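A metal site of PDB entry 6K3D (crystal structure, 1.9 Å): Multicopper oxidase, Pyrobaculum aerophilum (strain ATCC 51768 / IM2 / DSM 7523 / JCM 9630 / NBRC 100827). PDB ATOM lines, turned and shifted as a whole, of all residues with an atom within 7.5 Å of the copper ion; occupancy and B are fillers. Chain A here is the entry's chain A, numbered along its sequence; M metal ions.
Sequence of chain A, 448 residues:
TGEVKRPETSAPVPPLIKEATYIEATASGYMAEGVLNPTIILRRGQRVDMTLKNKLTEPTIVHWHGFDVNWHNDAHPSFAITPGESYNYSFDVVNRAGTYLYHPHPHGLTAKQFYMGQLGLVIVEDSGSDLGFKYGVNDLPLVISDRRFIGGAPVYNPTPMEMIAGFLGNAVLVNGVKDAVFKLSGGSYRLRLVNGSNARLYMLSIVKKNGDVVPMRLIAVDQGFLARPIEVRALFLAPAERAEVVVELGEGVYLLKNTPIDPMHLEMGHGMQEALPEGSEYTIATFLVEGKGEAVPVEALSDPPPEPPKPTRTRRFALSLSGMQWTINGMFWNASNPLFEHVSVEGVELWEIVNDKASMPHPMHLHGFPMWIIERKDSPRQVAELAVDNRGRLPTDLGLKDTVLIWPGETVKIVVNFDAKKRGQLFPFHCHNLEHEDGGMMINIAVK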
ATOM      1  N   ILE A 164      13.421  18.139  15.452  1.00  0.00           N
ATOM      2  CA  ILE A 164      12.067  18.694  15.370  1.00  0.00           C
ATOM      3  C   ILE A 164      11.748  19.134  13.944  1.00  0.00           C
ATOM      4  O   ILE A 164      10.646  18.924  13.442  1.00  0.00           O
ATOM      5  CB  ILE A 164      11.922  19.864  16.364  1.00  0.00           C
ATOM      6  CG1 ILE A 164      12.066  19.353  17.793  1.00  0.00           C
ATOM      7  CG2 ILE A 164      10.571  20.570  16.176  1.00  0.00           C
ATOM      8  CD1 ILE A 164      10.999  18.385  18.184  1.00  0.00           C
ATOM      9  N   ALA A 165      12.689  19.784  13.289  1.00  0.00           N
ATOM     10  CA  ALA A 165      12.401  20.414  12.010  1.00  0.00           C
ATOM     11  C   ALA A 165      12.745  19.536  10.811  1.00  0.00           C
ATOM     12  O   ALA A 165      12.204  19.753   9.723  1.00  0.00           O
ATOM     13  CB  ALA A 165      13.170  21.728  11.902  1.00  0.00           C
ATOM     14  N   LEU A 319      -2.203  16.046  13.431  1.00  0.00           N
ATOM     15  CA  LEU A 319      -0.749  16.072  13.454  1.00  0.00           C
ATOM     16  C   LEU A 319      -0.335  17.277  14.286  1.00  0.00           C
ATOM     17  O   LEU A 319      -0.710  18.408  13.950  1.00  0.00           O
ATOM     18  CB  LEU A 319      -0.165  16.137  12.050  1.00  0.00           C
ATOM     19  CG  LEU A 319      -0.756  15.143  11.034  1.00  0.00           C
ATOM     20  CD1 LEU A 319      -0.067  15.268   9.648  1.00  0.00           C
ATOM     21  CD2 LEU A 319      -0.679  13.709  11.568  1.00  0.00           C
ATOM     22  N   TRP A 326       6.790  14.925  18.190  1.00  0.00           N
ATOM     23  CA  TRP A 326       5.749  14.920  17.166  1.00  0.00           C
ATOM     24  C   TRP A 326       4.775  13.793  17.439  1.00  0.00           C
ATOM     25  O   TRP A 326       5.171  12.681  17.810  1.00  0.00           O
ATOM     26  CB  TRP A 326       6.359  14.744  15.781  1.00  0.00           C
ATOM     27  CG  TRP A 326       6.993  15.982  15.250  1.00  0.00           C
ATOM     28  CD1 TRP A 326       8.314  16.219  15.121  1.00  0.00           C
ATOM     29  CD2 TRP A 326       6.310  17.153  14.799  1.00  0.00           C
ATOM     30  NE1 TRP A 326       8.518  17.474  14.599  1.00  0.00           N
ATOM     31  CE2 TRP A 326       7.303  18.061  14.384  1.00  0.00           C
ATOM     32  CE3 TRP A 326       4.964  17.507  14.688  1.00  0.00           C
ATOM     33  CZ2 TRP A 326       6.978  19.314  13.863  1.00  0.00           C
ATOM     34  CZ3 TRP A 326       4.651  18.761  14.171  1.00  0.00           C
ATOM     35  CH2 TRP A 326       5.655  19.649  13.773  1.00  0.00           C
ATOM     36  N   ASN A 355      -3.510  18.742   9.782  1.00  0.00           N
ATOM     37  CA  ASN A 355      -2.216  19.213  10.273  1.00  0.00           C
ATOM     38  C   ASN A 355      -2.435  20.536  11.019  1.00  0.00           C
ATOM     39  O   ASN A 355      -3.070  21.458  10.489  1.00  0.00           O
ATOM     40  CB  ASN A 355      -1.226  19.398   9.123  1.00  0.00           C
ATOM     41  CG  ASN A 355       0.194  19.520   9.604  1.00  0.00           C
ATOM     42  OD1 ASN A 355       0.461  19.511  10.805  1.00  0.00           O
ATOM     43  ND2 ASN A 355       1.131  19.662   8.653  1.00  0.00           N
ATOM     44  N   SER A 359       2.730  23.973  12.974  1.00  0.00           N
ATOM     45  CA  SER A 359       3.286  22.689  12.560  1.00  0.00           C
ATOM     46  C   SER A 359       4.070  22.963  11.292  1.00  0.00           C
ATOM     47  O   SER A 359       4.298  24.117  10.920  1.00  0.00           O
ATOM     48  CB  SER A 359       2.163  21.665  12.371  1.00  0.00           C
ATOM     49  OG  SER A 359       2.657  20.370  12.008  1.00  0.00           O
ATOM     50  N   MET A 360       4.502  21.891  10.626  1.00  0.00           N
ATOM     51  CA  MET A 360       5.188  22.025   9.349  1.00  0.00           C
ATOM     52  C   MET A 360       4.623  20.960   8.410  1.00  0.00           C
ATOM     53  O   MET A 360       3.903  20.073   8.867  1.00  0.00           O
ATOM     54  CB  MET A 360       6.703  21.870   9.544  1.00  0.00           C
ATOM     55  CG  MET A 360       7.086  20.586  10.229  1.00  0.00           C
ATOM     56  SD  MET A 360       8.850  20.304  10.197  1.00  0.00           S
ATOM     57  CE  MET A 360       9.069  19.760   8.464  1.00  0.00           C
ATOM     58  N   PRO A 361       4.880  21.032   7.106  1.00  0.00           N
ATOM     59  CA  PRO A 361       4.324  20.008   6.220  1.00  0.00           C
ATOM     60  C   PRO A 361       4.842  18.626   6.631  1.00  0.00           C
ATOM     61  O   PRO A 361       6.012  18.469   6.972  1.00  0.00           O
ATOM     62  CB  PRO A 361       4.840  20.422   4.827  1.00  0.00           C
ATOM     63  CG  PRO A 361       5.185  21.892   4.949  1.00  0.00           C
ATOM     64  CD  PRO A 361       5.671  22.042   6.369  1.00  0.00           C
ATOM     65  N   HIS A 362       3.950  17.642   6.641  1.00  0.00           N
ATOM     66  CA  HIS A 362       4.309  16.261   6.986  1.00  0.00           C
ATOM     67  C   HIS A 362       3.956  15.339   5.822  1.00  0.00           C
ATOM     68  O   HIS A 362       2.774  15.267   5.441  1.00  0.00           O
ATOM     69  CB  HIS A 362       3.570  15.777   8.248  1.00  0.00           C
ATOM     70  CG  HIS A 362       3.869  16.557   9.493  1.00  0.00           C
ATOM     71  ND1 HIS A 362       5.063  16.447  10.173  1.00  0.00           N
ATOM     72  CD2 HIS A 362       3.115  17.438  10.206  1.00  0.00           C
ATOM     73  CE1 HIS A 362       5.048  17.228  11.237  1.00  0.00           C
ATOM     74  NE2 HIS A 362       3.876  17.842  11.277  1.00  0.00           N
ATOM     75  N   PRO A 363       4.928  14.618   5.234  1.00  0.00           N
ATOM     76  CA  PRO A 363       4.561  13.565   4.254  1.00  0.00           C
ATOM     77  C   PRO A 363       4.141  12.287   4.957  1.00  0.00           C
ATOM     78  O   PRO A 363       4.977  11.458   5.338  1.00  0.00           O
ATOM     79  CB  PRO A 363       5.842  13.388   3.451  1.00  0.00           C
ATOM     80  CG  PRO A 363       6.939  13.634   4.512  1.00  0.00           C
ATOM     81  CD  PRO A 363       6.389  14.784   5.347  1.00  0.00           C
ATOM     82  N   MET A 364       2.838  12.090   5.134  1.00  0.00           N
ATOM     83  CA  MET A 364       2.359  10.981   5.935  1.00  0.00           C
ATOM     84  C   MET A 364       2.278   9.728   5.070  1.00  0.00           C
ATOM     85  O   MET A 364       1.806   9.775   3.938  1.00  0.00           O
ATOM     86  CB  MET A 364       0.997  11.299   6.553  1.00  0.00           C
ATOM     87  CG  MET A 364       1.033  12.440   7.610  1.00  0.00           C
ATOM     88  SD  MET A 364       2.237  12.135   8.908  1.00  0.00           S
ATOM     89  CE  MET A 364       1.610  10.665   9.693  1.00  0.00           C
ATOM     90  N   HIS A 430       3.112   6.692   9.674  1.00  0.00           N
ATOM     91  CA  HIS A 430       4.135   7.592  10.172  1.00  0.00           C
ATOM     92  C   HIS A 430       4.464   8.682   9.170  1.00  0.00           C
ATOM     93  O   HIS A 430       4.135   8.591   7.983  1.00  0.00           O
ATOM     94  CB  HIS A 430       5.421   6.835  10.519  1.00  0.00           C
ATOM     95  CG  HIS A 430       6.154   6.298   9.325  1.00  0.00           C
ATOM     96  ND1 HIS A 430       7.135   7.008   8.680  1.00  0.00           N
ATOM     97  CD2 HIS A 430       6.055   5.113   8.696  1.00  0.00           C
ATOM     98  CE1 HIS A 430       7.614   6.289   7.680  1.00  0.00           C
ATOM     99  NE2 HIS A 430       6.967   5.136   7.665  1.00  0.00           N
ATOM    100  N   CYS A 431       5.139   9.711   9.661  1.00  0.00           N
ATOM    101  CA  CYS A 431       5.674  10.731   8.778  1.00  0.00           C
ATOM    102  C   CYS A 431       6.963  10.242   8.134  1.00  0.00           C
ATOM    103  O   CYS A 431       7.784   9.590   8.796  1.00  0.00           O
ATOM    104  CB  CYS A 431       5.943  12.026   9.549  1.00  0.00           C
ATOM    105  SG  CYS A 431       6.572  13.298   8.444  1.00  0.00           S
ATOM    106  N   HIS A 432       7.135  10.534   6.849  1.00  0.00           N
ATOM    107  CA  HIS A 432       8.335  10.095   6.178  1.00  0.00           C
ATOM    108  C   HIS A 432       9.443  11.130   6.174  1.00  0.00           C
ATOM    109  O   HIS A 432      10.447  10.951   5.475  1.00  0.00           O
ATOM    110  CB  HIS A 432       8.034   9.656   4.747  1.00  0.00           C
ATOM    111  CG  HIS A 432       8.856   8.483   4.345  1.00  0.00           C
ATOM    112  ND1 HIS A 432      10.209   8.592   4.077  1.00  0.00           N
ATOM    113  CD2 HIS A 432       8.558   7.173   4.264  1.00  0.00           C
ATOM    114  CE1 HIS A 432      10.691   7.396   3.792  1.00  0.00           C
ATOM    115  NE2 HIS A 432       9.714   6.521   3.914  1.00  0.00           N
ATOM    116  N   ASN A 433       9.289  12.223   6.926  1.00  0.00           N
ATOM    117  CA  ASN A 433      10.431  13.015   7.349  1.00  0.00           C
ATOM    118  C   ASN A 433      11.213  12.160   8.341  1.00  0.00           C
ATOM    119  O   ASN A 433      10.698  11.808   9.416  1.00  0.00           O
ATOM    120  CB  ASN A 433       9.925  14.337   7.956  1.00  0.00           C
ATOM    121  CG  ASN A 433      11.035  15.177   8.575  1.00  0.00           C
ATOM    122  OD1 ASN A 433      11.945  14.676   9.230  1.00  0.00           O
ATOM    123  ND2 ASN A 433      10.930  16.498   8.390  1.00  0.00           N
ATOM    124  N   LEU A 434      12.411  11.728   7.966  1.00  0.00           N
ATOM    125  CA  LEU A 434      13.059  10.665   8.722  1.00  0.00           C
ATOM    126  C   LEU A 434      13.469  11.115  10.120  1.00  0.00           C
ATOM    127  O   LEU A 434      13.574  10.287  11.029  1.00  0.00           O
ATOM    128  CB  LEU A 434      14.260  10.107   7.956  1.00  0.00           C
ATOM    129  CG  LEU A 434      13.888   9.447   6.616  1.00  0.00           C
ATOM    130  CD1 LEU A 434      15.126   8.787   6.038  1.00  0.00           C
ATOM    131  CD2 LEU A 434      12.780   8.430   6.808  1.00  0.00           C
ATOM    132  N   GLU A 435      13.702  12.414  10.324  1.00  0.00           N
ATOM    133  CA  GLU A 435      13.932  12.903  11.681  1.00  0.00           C
ATOM    134  C   GLU A 435      12.660  12.831  12.512  1.00  0.00           C
ATOM    135  O   GLU A 435      12.708  12.451  13.694  1.00  0.00           O
ATOM    136  CB  GLU A 435      14.455  14.346  11.633  1.00  0.00           C
ATOM    137  CG  GLU A 435      15.921  14.466  11.283  1.00  0.00           C
ATOM    138  CD  GLU A 435      16.217  14.059   9.845  1.00  0.00           C
ATOM    139  OE1 GLU A 435      15.662  14.685   8.910  1.00  0.00           O
ATOM    140  OE2 GLU A 435      17.034  13.135   9.647  1.00  0.00           O
ATOM    141  N   HIS A 436      11.519  13.171  11.918  1.00  0.00           N
ATOM    142  CA  HIS A 436      10.243  12.979  12.609  1.00  0.00           C
ATOM    143  C   HIS A 436      10.010  11.495  12.912  1.00  0.00           C
ATOM    144  O   HIS A 436       9.536  11.134  13.996  1.00  0.00           O
ATOM    145  CB  HIS A 436       9.099  13.551  11.771  1.00  0.00           C
ATOM    146  CG  HIS A 436       9.159  15.053  11.589  1.00  0.00           C
ATOM    147  ND1 HIS A 436       8.199  15.755  10.896  1.00  0.00           N
ATOM    148  CD2 HIS A 436      10.078  15.973  11.998  1.00  0.00           C
ATOM    149  CE1 HIS A 436       8.507  17.046  10.899  1.00  0.00           C
ATOM    150  NE2 HIS A 436       9.648  17.205  11.555  1.00  0.00           N
ATOM    151  N   GLU A 437      10.336  10.625  11.948  1.00  0.00           N
ATOM    152  CA  GLU A 437      10.145   9.202  12.130  1.00  0.00           C
ATOM    153  C   GLU A 437      11.031   8.657  13.236  1.00  0.00           C
ATOM    154  O   GLU A 437      10.547   7.987  14.148  1.00  0.00           O
ATOM    155  CB  GLU A 437      10.419   8.475  10.822  1.00  0.00           C
ATOM    156  CG  GLU A 437      10.088   6.983  10.891  1.00  0.00           C
ATOM    157  CD  GLU A 437      10.505   6.285   9.623  1.00  0.00           C
ATOM    158  OE1 GLU A 437      10.386   6.934   8.557  1.00  0.00           O
ATOM    159  OE2 GLU A 437      10.966   5.127   9.682  1.00  0.00           O
ATOM    160  N   MET A 441       7.436   9.892  15.409  1.00  0.00           N
ATOM    161  CA  MET A 441       6.171  10.262  14.788  1.00  0.00           C
ATOM    162  C   MET A 441       5.709   9.067  13.937  1.00  0.00           C
ATOM    163  O   MET A 441       5.708   9.097  12.711  1.00  0.00           O
ATOM    164  CB  MET A 441       6.317  11.530  13.948  1.00  0.00           C
ATOM    165  CG  MET A 441       4.979  12.147  13.516  1.00  0.00           C
ATOM    166  SD  MET A 441       5.162  13.706  12.608  1.00  0.00           S
ATOM    167  CE  MET A 441       3.452  14.131  12.276  1.00  0.00           C
HETATM  168 CU    CU M   1       6.609  15.036   9.870  1.00  0.00          CU
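The backbone carbonyl oxygen (O) of His 436 sits at hydrogen-bond distance from the backbone NH (N) of Met 441 (2.8 Å). OD1 of Asn 433 is in hydrogen-bond range of N of His 436 (3.1 Å). A ring nitrogen (NE2) of His 436 sits at hydrogen-bond distance from the backbone carbonyl oxygen (O) of Ile 164 (2.7 Å). A ring nitrogen (ND1) of His 362 sits close to the side-chain sulfur (SD) of Met 441, 3.7 Å away. NE2 of His 362 lies close to O of Met 360, at 3.3 Å. The side-chain hydroxyl of Ser 359 is in hydrogen-bond range of a ring nitrogen (NE2) of His 362. N of Cys 431 sits at hydrogen-bond distance from O of Met 441, at 3.2 Å. The side-chain sulfur (SG) of Cys 431 lies close to the backbone NH (N) of Asn 433 (3.3 Å).
Asn 433 touches the copper ion. SD of Met 441 touches the copper ion (3.4 Å). Of the 20 residues printed, 5 come within 4 Å of the copper ion.
The copper ion is bound by a ring nitrogen (ND1) of His 436 (2.0 Å), a ring nitrogen (ND1) of His 362 (2.1 Å) and the side-chain sulfur of Cys 431 (2.2 Å). The copper ion has three donor atoms within binding distance.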
